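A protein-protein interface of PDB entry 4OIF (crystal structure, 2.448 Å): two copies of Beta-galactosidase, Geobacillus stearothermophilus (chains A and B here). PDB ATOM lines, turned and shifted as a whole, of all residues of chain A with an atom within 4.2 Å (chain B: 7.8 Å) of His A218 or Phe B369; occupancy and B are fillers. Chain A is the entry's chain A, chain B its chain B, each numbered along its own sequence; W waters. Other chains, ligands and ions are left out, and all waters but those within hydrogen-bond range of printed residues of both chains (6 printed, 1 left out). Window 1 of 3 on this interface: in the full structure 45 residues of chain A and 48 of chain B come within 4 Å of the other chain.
Of the printed residues of chain B, His A218 touches Ser B368, Phe B369 and Lys B371.
Gly A219 touches none of the printed residues of chain B.
Asn A221 touches none of the printed residues of chain B.
Of the printed residues of chain B, Asp A510 touches Lys B371.
Of the printed residues of chain A, Trp B330 touches Gln A429.
Of chain A, only Phe A195, Trp A196, Thr A216, His A218 and Gln A429 come within 4 Å of Phe B369.
His B373 touches none of the printed residues of chain A.
The nearest residue of chain B that does not touch His A218 is Glu B370 (5.1 Å).
The nearest printed residue of chain A that does not touch Phe B369 is Ile A217 (5.1 Å).
The side-chain amide nitrogen of Asn A221 is in hydrogen-bond range of the backbone carbonyl oxygen of Ile A217 (3.2 Å).
A ring nitrogen (ND1) of His A218 is in hydrogen-bond range of the side-chain carboxylate of Asp A427, at 2.8 Å.
The guanidinium group (NH2) of Arg B119 lies within salt-bridge range of the side-chain carboxylate (OE2) of Glu B370 (3.97 Å).
The side-chain amide nitrogen (ND2) of Asn B329 sits at hydrogen-bond distance from the backbone carbonyl oxygen (O) of Phe B369, 3.1 Å away.
No position is printed for both chains.
Of the 18 pairs that touch across the chains among the printed residues, none has its exchanged pair printed and touching as well.
Printed residues of chain B that touch a printed residue of chain A: Arg B119, Asn B329, Trp B330, Ser B365, Ser B368, Phe B369, Glu B370, Lys B371 and Phe B372.
Hydrophobic or aromatic side chains of chain A within 4 Å of the printed part of chain B: Phe A195, Trp A196 and His A218.
Among the printed residues, 18 pairs touch across the chains.
Among the printed residues, Asp or Glu carboxylates within 4 Å of a Lys or Arg side-chain nitrogen of the other chain: Asp A510 with Lys B371 (2.6 Å).
Ser B368 touches Phe A195.
Phe B369 touches Phe A195 (CB to CE2, 3.8 Å).
OE1 of Glu B370 touches CZ of Phe A195, 3.3 Å away.
Phe B369 touches Trp A196.
Trp A196 touches Glu B370 (CZ2 to OE2, 3.6 Å).
His A218 touches Phe B369.
His A218 touches Lys B371.
OE1 of Gln A429 touches CA of Trp B330, at 3.6 Å.
O of Phe B369 touches CB of Gln A429, 3.3 Å away.
Gln A429 touches Phe B372 (O to CB, 3.5 Å).
Water W3 lies within hydrogen-bond range of O of Gln A429 (2.6 Å), N of Phe B372 (2.8 Å), O of Phe B369 (2.9 Å) and N of Lys B371 (3.3 Å).
Water W6 bridges the backbone carbonyl oxygen (O) of Asp A510 (2.7 Å) and the backbone NH (N) of Ser B368 (2.9 Å).
Water W5 lies within hydrogen-bond range of a ring nitrogen (NE2) of His A218 (2.7 Å), the backbone NH of Gln A429 (2.9 Å) and the side-chain amino group of Lys B371 (3.0 Å).
Water W2 bridges O of Phe A195 (2.8 Å) and OG of Ser B368 (2.9 Å).
Water W1 lies within hydrogen-bond range of the side-chain hydroxyl (OG1) of Thr A216 (2.8 Å) and the side-chain hydroxyl (OG) of Ser B368 (2.9 Å).
Water W4 lies within hydrogen-bond range of the side-chain carboxylate (OE1) of Glu B370, the indole nitrogen (NE1) of Trp A196 and the guanidinium group (NH1) of Arg B119.
The side-chain hydroxyl (OG) of Ser B368 lies within hydrogen-bond range of the backbone carbonyl oxygen (O) of Thr A216.
The backbone NH (N) of Phe B369 lies close to the backbone carbonyl oxygen (O) of Thr A216, at 3.3 Å.
NE2 of His A218 lies close to O of Ser B368, 3.4 Å away.
OE1 of Gln A429 lies close to O of Asn B329 (3.5 Å).
The side-chain carboxylate (OD2) of Asp A510 lies within salt-bridge range of the side-chain amino group (NZ) of Lys B371.
The indole nitrogen of Trp A196 lies close to the guanidinium group of Arg B119, at 3.0 Å.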
ATOM      1  N   PHE A 195     -33.049 -27.131  20.528  1.00  0.00           N
ATOM      2  CA  PHE A 195     -33.340 -26.876  21.931  1.00  0.00           C
ATOM      3  C   PHE A 195     -34.220 -25.625  22.093  1.00  0.00           C
ATOM      4  O   PHE A 195     -33.901 -24.559  21.565  1.00  0.00           O
ATOM      5  CB  PHE A 195     -32.016 -26.730  22.695  1.00  0.00           C
ATOM      6  CG  PHE A 195     -32.176 -26.409  24.146  1.00  0.00           C
ATOM      7  CD1 PHE A 195     -32.524 -27.396  25.055  1.00  0.00           C
ATOM      8  CD2 PHE A 195     -31.966 -25.116  24.610  1.00  0.00           C
ATOM      9  CE1 PHE A 195     -32.669 -27.102  26.403  1.00  0.00           C
ATOM     10  CE2 PHE A 195     -32.107 -24.818  25.962  1.00  0.00           C
ATOM     11  CZ  PHE A 195     -32.460 -25.812  26.856  1.00  0.00           C
ATOM     12  N   TRP A 196     -35.334 -25.773  22.806  1.00  0.00           N
ATOM     13  CA  TRP A 196     -36.284 -24.676  23.032  1.00  0.00           C
ATOM     14  C   TRP A 196     -36.842 -24.094  21.728  1.00  0.00           C
ATOM     15  O   TRP A 196     -37.187 -22.916  21.662  1.00  0.00           O
ATOM     16  CB  TRP A 196     -35.640 -23.564  23.876  1.00  0.00           C
ATOM     17  CG  TRP A 196     -35.478 -23.952  25.316  1.00  0.00           C
ATOM     18  CD1 TRP A 196     -35.890 -25.106  25.897  1.00  0.00           C
ATOM     19  CD2 TRP A 196     -34.853 -23.184  26.348  1.00  0.00           C
ATOM     20  NE1 TRP A 196     -35.564 -25.113  27.231  1.00  0.00           N
ATOM     21  CE2 TRP A 196     -34.928 -23.940  27.535  1.00  0.00           C
ATOM     22  CE3 TRP A 196     -34.225 -21.936  26.382  1.00  0.00           C
ATOM     23  CZ2 TRP A 196     -34.394 -23.491  28.744  1.00  0.00           C
ATOM     24  CZ3 TRP A 196     -33.700 -21.490  27.590  1.00  0.00           C
ATOM     25  CH2 TRP A 196     -33.786 -22.265  28.749  1.00  0.00           C
ATOM     26  N   THR A 216     -29.885 -17.085  25.304  1.00  0.00           N
ATOM     27  CA  THR A 216     -29.777 -18.453  25.803  1.00  0.00           C
ATOM     28  C   THR A 216     -29.187 -19.425  24.772  1.00  0.00           C
ATOM     29  O   THR A 216     -29.096 -20.632  25.031  1.00  0.00           O
ATOM     30  CB  THR A 216     -31.157 -19.004  26.243  1.00  0.00           C
ATOM     31  OG1 THR A 216     -32.010 -19.147  25.095  1.00  0.00           O
ATOM     32  CG2 THR A 216     -31.812 -18.072  27.244  1.00  0.00           C
ATOM     33  N   ILE A 217     -28.799 -18.918  23.604  1.00  0.00           N
ATOM     34  CA  ILE A 217     -28.104 -19.754  22.624  1.00  0.00           C
ATOM     35  C   ILE A 217     -26.607 -19.420  22.633  1.00  0.00           C
ATOM     36  O   ILE A 217     -26.194 -18.364  22.158  1.00  0.00           O
ATOM     37  CB  ILE A 217     -28.681 -19.590  21.196  1.00  0.00           C
ATOM     38  CG1 ILE A 217     -30.211 -19.697  21.196  1.00  0.00           C
ATOM     39  CG2 ILE A 217     -28.095 -20.635  20.262  1.00  0.00           C
ATOM     40  CD1 ILE A 217     -30.845 -19.509  19.804  1.00  0.00           C
ATOM     41  N   HIS A 218     -25.806 -20.329  23.184  1.00  0.00           N
ATOM     42  CA  HIS A 218     -24.380 -20.104  23.366  1.00  0.00           C
ATOM     43  C   HIS A 218     -23.660 -19.838  22.048  1.00  0.00           C
ATOM     44  O   HIS A 218     -22.805 -18.963  21.972  1.00  0.00           O
ATOM     45  CB  HIS A 218     -23.728 -21.302  24.064  1.00  0.00           C
ATOM     46  CG  HIS A 218     -24.203 -21.529  25.470  1.00  0.00           C
ATOM     47  ND1 HIS A 218     -24.108 -20.567  26.455  1.00  0.00           N
ATOM     48  CD2 HIS A 218     -24.754 -22.618  26.060  1.00  0.00           C
ATOM     49  CE1 HIS A 218     -24.591 -21.052  27.588  1.00  0.00           C
ATOM     50  NE2 HIS A 218     -24.998 -22.291  27.374  1.00  0.00           N
ATOM     51  N   GLY A 219     -24.005 -20.592  21.014  1.00  0.00           N
ATOM     52  CA  GLY A 219     -23.335 -20.469  19.727  1.00  0.00           C
ATOM     53  C   GLY A 219     -23.585 -19.116  19.098  1.00  0.00           C
ATOM     54  O   GLY A 219     -22.705 -18.546  18.450  1.00  0.00           O
ATOM     55  N   LEU A 220     -24.796 -18.596  19.303  1.00  0.00           N
ATOM     56  CA  LEU A 220     -25.129 -17.246  18.874  1.00  0.00           C
ATOM     57  C   LEU A 220     -24.292 -16.235  19.649  1.00  0.00           C
ATOM     58  O   LEU A 220     -23.739 -15.319  19.061  1.00  0.00           O
ATOM     59  CB  LEU A 220     -26.624 -16.961  19.053  1.00  0.00           C
ATOM     60  CG  LEU A 220     -27.083 -15.501  18.925  1.00  0.00           C
ATOM     61  CD1 LEU A 220     -26.655 -14.875  17.595  1.00  0.00           C
ATOM     62  CD2 LEU A 220     -28.592 -15.371  19.108  1.00  0.00           C
ATOM     63  N   ASN A 221     -24.193 -16.393  20.963  1.00  0.00           N
ATOM     64  CA  ASN A 221     -23.410 -15.453  21.765  1.00  0.00           C
ATOM     65  C   ASN A 221     -21.937 -15.405  21.322  1.00  0.00           C
ATOM     66  O   ASN A 221     -21.346 -14.320  21.118  1.00  0.00           O
ATOM     67  CB  ASN A 221     -23.516 -15.819  23.248  1.00  0.00           C
ATOM     68  CG  ASN A 221     -24.947 -15.843  23.738  1.00  0.00           C
ATOM     69  OD1 ASN A 221     -25.787 -15.096  23.252  1.00  0.00           O
ATOM     70  ND2 ASN A 221     -25.227 -16.688  24.712  1.00  0.00           N
ATOM     71  N   LEU A 222     -21.373 -16.598  21.149  1.00  0.00           N
ATOM     72  CA  LEU A 222     -19.993 -16.778  20.722  1.00  0.00           C
ATOM     73  C   LEU A 222     -19.757 -16.172  19.335  1.00  0.00           C
ATOM     74  O   LEU A 222     -18.889 -15.307  19.160  1.00  0.00           O
ATOM     75  CB  LEU A 222     -19.650 -18.267  20.729  1.00  0.00           C
ATOM     76  CG  LEU A 222     -18.219 -18.707  20.415  1.00  0.00           C
ATOM     77  CD1 LEU A 222     -17.204 -18.034  21.336  1.00  0.00           C
ATOM     78  CD2 LEU A 222     -18.125 -20.226  20.534  1.00  0.00           C
ATOM     79  N   ASP A 427     -19.691 -17.728  29.336  1.00  0.00           N
ATOM     80  CA  ASP A 427     -21.104 -17.785  28.977  1.00  0.00           C
ATOM     81  C   ASP A 427     -21.814 -19.070  29.397  1.00  0.00           C
ATOM     82  O   ASP A 427     -23.039 -19.094  29.515  1.00  0.00           O
ATOM     83  CB  ASP A 427     -21.273 -17.619  27.472  1.00  0.00           C
ATOM     84  CG  ASP A 427     -22.674 -17.221  27.102  1.00  0.00           C
ATOM     85  OD1 ASP A 427     -23.146 -16.207  27.655  1.00  0.00           O
ATOM     86  OD2 ASP A 427     -23.310 -17.927  26.282  1.00  0.00           O
ATOM     87  N   ALA A 428     -21.045 -20.128  29.614  1.00  0.00           N
ATOM     88  CA  ALA A 428     -21.602 -21.455  29.879  1.00  0.00           C
ATOM     89  C   ALA A 428     -22.446 -21.518  31.153  1.00  0.00           C
ATOM     90  O   ALA A 428     -22.113 -20.919  32.171  1.00  0.00           O
ATOM     91  CB  ALA A 428     -20.472 -22.491  29.938  1.00  0.00           C
ATOM     92  N   GLN A 429     -23.556 -22.239  31.080  1.00  0.00           N
ATOM     93  CA  GLN A 429     -24.374 -22.498  32.254  1.00  0.00           C
ATOM     94  C   GLN A 429     -23.888 -23.784  32.921  1.00  0.00           C
ATOM     95  O   GLN A 429     -24.109 -24.893  32.410  1.00  0.00           O
ATOM     96  CB  GLN A 429     -25.851 -22.597  31.873  1.00  0.00           C
ATOM     97  CG  GLN A 429     -26.437 -21.270  31.455  1.00  0.00           C
ATOM     98  CD  GLN A 429     -26.583 -20.305  32.624  1.00  0.00           C
ATOM     99  OE1 GLN A 429     -27.069 -20.673  33.693  1.00  0.00           O
ATOM    100  NE2 GLN A 429     -26.158 -19.070  32.427  1.00  0.00           N
ATOM    101  N   ASP A 510     -18.867 -24.464  20.933  1.00  0.00           N
ATOM    102  CA  ASP A 510     -19.383 -24.757  22.269  1.00  0.00           C
ATOM    103  C   ASP A 510     -20.332 -25.974  22.216  1.00  0.00           C
ATOM    104  O   ASP A 510     -21.320 -26.072  22.944  1.00  0.00           O
ATOM    105  CB  ASP A 510     -20.071 -23.530  22.885  1.00  0.00           C
ATOM    106  CG  ASP A 510     -20.258 -23.663  24.404  1.00  0.00           C
ATOM    107  OD1 ASP A 510     -19.291 -24.034  25.110  1.00  0.00           O
ATOM    108  OD2 ASP A 510     -21.386 -23.427  24.890  1.00  0.00           O
ATOM    109  N   ARG B 119     -37.948 -18.615  26.134  1.00  0.00           N
ATOM    110  CA  ARG B 119     -39.093 -19.515  26.181  1.00  0.00           C
ATOM    111  C   ARG B 119     -40.077 -19.026  27.235  1.00  0.00           C
ATOM    112  O   ARG B 119     -39.781 -18.074  27.946  1.00  0.00           O
ATOM    113  CB  ARG B 119     -38.650 -20.945  26.505  1.00  0.00           C
ATOM    114  CG  ARG B 119     -38.329 -21.142  27.981  1.00  0.00           C
ATOM    115  CD  ARG B 119     -37.806 -22.514  28.288  1.00  0.00           C
ATOM    116  NE  ARG B 119     -37.341 -22.600  29.667  1.00  0.00           N
ATOM    117  CZ  ARG B 119     -37.098 -23.739  30.311  1.00  0.00           C
ATOM    118  NH1 ARG B 119     -37.253 -24.908  29.698  1.00  0.00           N
ATOM    119  NH2 ARG B 119     -36.685 -23.705  31.570  1.00  0.00           N
ATOM    120  N   ASN B 329     -27.952 -26.669  35.835  1.00  0.00           N
ATOM    121  CA  ASN B 329     -27.043 -25.873  35.030  1.00  0.00           C
ATOM    122  C   ASN B 329     -27.043 -24.434  35.486  1.00  0.00           C
ATOM    123  O   ASN B 329     -26.132 -23.689  35.166  1.00  0.00           O
ATOM    124  CB  ASN B 329     -27.455 -25.921  33.563  1.00  0.00           C
ATOM    125  CG  ASN B 329     -28.844 -25.318  33.348  1.00  0.00           C
ATOM    126  OD1 ASN B 329     -29.795 -25.698  34.031  1.00  0.00           O
ATOM    127  ND2 ASN B 329     -28.950 -24.335  32.453  1.00  0.00           N
ATOM    128  N   TRP B 330     -28.074 -24.048  36.236  1.00  0.00           N
ATOM    129  CA  TRP B 330     -28.405 -22.632  36.389  1.00  0.00           C
ATOM    130  C   TRP B 330     -28.269 -22.107  37.812  1.00  0.00           C
ATOM    131  O   TRP B 330     -28.644 -20.958  38.080  1.00  0.00           O
ATOM    132  CB  TRP B 330     -29.842 -22.373  35.896  1.00  0.00           C
ATOM    133  CG  TRP B 330     -30.859 -23.162  36.667  1.00  0.00           C
ATOM    134  CD1 TRP B 330     -31.247 -24.445  36.428  1.00  0.00           C
ATOM    135  CD2 TRP B 330     -31.588 -22.728  37.820  1.00  0.00           C
ATOM    136  NE1 TRP B 330     -32.180 -24.838  37.354  1.00  0.00           N
ATOM    137  CE2 TRP B 330     -32.410 -23.802  38.221  1.00  0.00           C
ATOM    138  CE3 TRP B 330     -31.637 -21.534  38.545  1.00  0.00           C
ATOM    139  CZ2 TRP B 330     -33.269 -23.719  39.325  1.00  0.00           C
ATOM    140  CZ3 TRP B 330     -32.498 -21.452  39.642  1.00  0.00           C
ATOM    141  CH2 TRP B 330     -33.296 -22.540  40.021  1.00  0.00           C
ATOM    142  N   SER B 365     -28.580 -32.304  26.345  1.00  0.00           N
ATOM    143  CA  SER B 365     -28.504 -31.605  25.071  1.00  0.00           C
ATOM    144  C   SER B 365     -27.041 -31.351  24.730  1.00  0.00           C
ATOM    145  O   SER B 365     -26.249 -31.000  25.602  1.00  0.00           O
ATOM    146  CB  SER B 365     -29.281 -30.287  25.122  1.00  0.00           C
ATOM    147  OG  SER B 365     -30.644 -30.498  25.452  1.00  0.00           O
ATOM    148  N   ARG B 366     -26.672 -31.532  23.468  1.00  0.00           N
ATOM    149  CA  ARG B 366     -25.263 -31.405  23.121  1.00  0.00           C
ATOM    150  C   ARG B 366     -24.803 -29.948  23.170  1.00  0.00           C
ATOM    151  O   ARG B 366     -23.640 -29.654  23.467  1.00  0.00           O
ATOM    152  CB  ARG B 366     -24.985 -32.002  21.746  1.00  0.00           C
ATOM    153  CG  ARG B 366     -23.517 -31.942  21.390  1.00  0.00           C
ATOM    154  CD  ARG B 366     -23.237 -32.518  20.037  1.00  0.00           C
ATOM    155  NE  ARG B 366     -21.802 -32.552  19.793  1.00  0.00           N
ATOM    156  CZ  ARG B 366     -21.254 -32.984  18.667  1.00  0.00           C
ATOM    157  NH1 ARG B 366     -22.032 -33.422  17.689  1.00  0.00           N
ATOM    158  NH2 ARG B 366     -19.933 -32.978  18.521  1.00  0.00           N
ATOM    159  N   GLY B 367     -25.719 -29.033  22.880  1.00  0.00           N
ATOM    160  CA  GLY B 367     -25.398 -27.621  22.948  1.00  0.00           C
ATOM    161  C   GLY B 367     -26.504 -26.797  23.569  1.00  0.00           C
ATOM    162  O   GLY B 367     -27.517 -27.347  24.047  1.00  0.00           O
ATOM    163  N   SER B 368     -26.276 -25.483  23.573  1.00  0.00           N
ATOM    164  CA  SER B 368     -27.239 -24.484  24.029  1.00  0.00           C
ATOM    165  C   SER B 368     -27.357 -24.470  25.572  1.00  0.00           C
ATOM    166  O   SER B 368     -26.591 -25.142  26.286  1.00  0.00           O
ATOM    167  CB  SER B 368     -28.609 -24.716  23.368  1.00  0.00           C
ATOM    168  OG  SER B 368     -29.295 -23.486  23.222  1.00  0.00           O
ATOM    169  N   PHE B 369     -28.341 -23.727  26.065  1.00  0.00           N
ATOM    170  CA  PHE B 369     -28.369 -23.263  27.453  1.00  0.00           C
ATOM    171  C   PHE B 369     -28.273 -24.346  28.524  1.00  0.00           C
ATOM    172  O   PHE B 369     -27.738 -24.095  29.602  1.00  0.00           O
ATOM    173  CB  PHE B 369     -29.645 -22.451  27.685  1.00  0.00           C
ATOM    174  CG  PHE B 369     -29.517 -21.407  28.766  1.00  0.00           C
ATOM    175  CD1 PHE B 369     -28.733 -20.276  28.569  1.00  0.00           C
ATOM    176  CD2 PHE B 369     -30.188 -21.550  29.978  1.00  0.00           C
ATOM    177  CE1 PHE B 369     -28.614 -19.297  29.557  1.00  0.00           C
ATOM    178  CE2 PHE B 369     -30.075 -20.575  30.976  1.00  0.00           C
ATOM    179  CZ  PHE B 369     -29.286 -19.446  30.760  1.00  0.00           C
ATOM    180  N   GLU B 370     -28.792 -25.540  28.250  1.00  0.00           N
ATOM    181  CA  GLU B 370     -28.833 -26.564  29.285  1.00  0.00           C
ATOM    182  C   GLU B 370     -28.001 -27.792  28.947  1.00  0.00           C
ATOM    183  O   GLU B 370     -28.249 -28.871  29.472  1.00  0.00           O
ATOM    184  CB  GLU B 370     -30.286 -26.967  29.571  1.00  0.00           C
ATOM    185  CG  GLU B 370     -31.066 -25.908  30.359  1.00  0.00           C
ATOM    186  CD  GLU B 370     -32.544 -26.257  30.552  1.00  0.00           C
ATOM    187  OE1 GLU B 370     -33.060 -27.158  29.863  1.00  0.00           O
ATOM    188  OE2 GLU B 370     -33.204 -25.615  31.389  1.00  0.00           O
ATOM    189  N   LYS B 371     -26.993 -27.626  28.099  1.00  0.00           N
ATOM    190  CA  LYS B 371     -26.106 -28.738  27.765  1.00  0.00           C
ATOM    191  C   LYS B 371     -25.371 -29.333  28.986  1.00  0.00           C
ATOM    192  O   LYS B 371     -24.940 -30.489  28.936  1.00  0.00           O
ATOM    193  CB  LYS B 371     -25.081 -28.309  26.699  1.00  0.00           C
ATOM    194  CG  LYS B 371     -23.944 -27.401  27.178  1.00  0.00           C
ATOM    195  CD  LYS B 371     -23.142 -26.897  25.969  1.00  0.00           C
ATOM    196  CE  LYS B 371     -21.785 -26.289  26.366  1.00  0.00           C
ATOM    197  NZ  LYS B 371     -21.871 -24.936  26.986  1.00  0.00           N
ATOM    198  N   PHE B 372     -25.235 -28.575  30.076  1.00  0.00           N
ATOM    199  CA  PHE B 372     -24.619 -29.133  31.287  1.00  0.00           C
ATOM    200  C   PHE B 372     -25.628 -29.358  32.417  1.00  0.00           C
ATOM    201  O   PHE B 372     -25.240 -29.634  33.558  1.00  0.00           O
ATOM    202  CB  PHE B 372     -23.467 -28.243  31.764  1.00  0.00           C
ATOM    203  CG  PHE B 372     -22.327 -28.182  30.794  1.00  0.00           C
ATOM    204  CD1 PHE B 372     -22.018 -29.280  30.009  1.00  0.00           C
ATOM    205  CD2 PHE B 372     -21.579 -27.031  30.643  1.00  0.00           C
ATOM    206  CE1 PHE B 372     -20.977 -29.236  29.091  1.00  0.00           C
ATOM    207  CE2 PHE B 372     -20.530 -26.980  29.727  1.00  0.00           C
ATOM    208  CZ  PHE B 372     -20.229 -28.087  28.953  1.00  0.00           C
ATOM    209  N   HIS B 373     -26.918 -29.260  32.096  1.00  0.00           N
ATOM    210  CA  HIS B 373     -27.950 -29.694  33.030  1.00  0.00           C
ATOM    211  C   HIS B 373     -27.870 -31.203  33.158  1.00  0.00           C
ATOM    212  O   HIS B 373     -27.572 -31.891  32.193  1.00  0.00           O
ATOM    213  CB  HIS B 373     -29.362 -29.285  32.574  1.00  0.00           C
ATOM    214  CG  HIS B 373     -30.404 -29.433  33.645  1.00  0.00           C
ATOM    215  ND1 HIS B 373     -30.889 -30.659  34.055  1.00  0.00           N
ATOM    216  CD2 HIS B 373     -31.039 -28.508  34.406  1.00  0.00           C
ATOM    217  CE1 HIS B 373     -31.782 -30.482  35.012  1.00  0.00           C
ATOM    218  NE2 HIS B 373     -31.898 -29.186  35.238  1.00  0.00           N
HETATM  219  O   HOH W   1     -31.483 -21.625  23.849  1.00  0.00           O
HETATM  220  O   HOH W   2     -31.331 -23.531  21.137  1.00  0.00           O
HETATM  221  O   HOH W   3     -25.441 -25.780  30.302  1.00  0.00           O
HETATM  222  O   HOH W   4     -35.767 -27.407  29.037  1.00  0.00           O
HETATM  223  O   HOH W   5     -23.955 -24.224  28.963  1.00  0.00           O
HETATM  224  O   HOH W   6     -23.554 -24.659  23.180  1.00  0.00           O
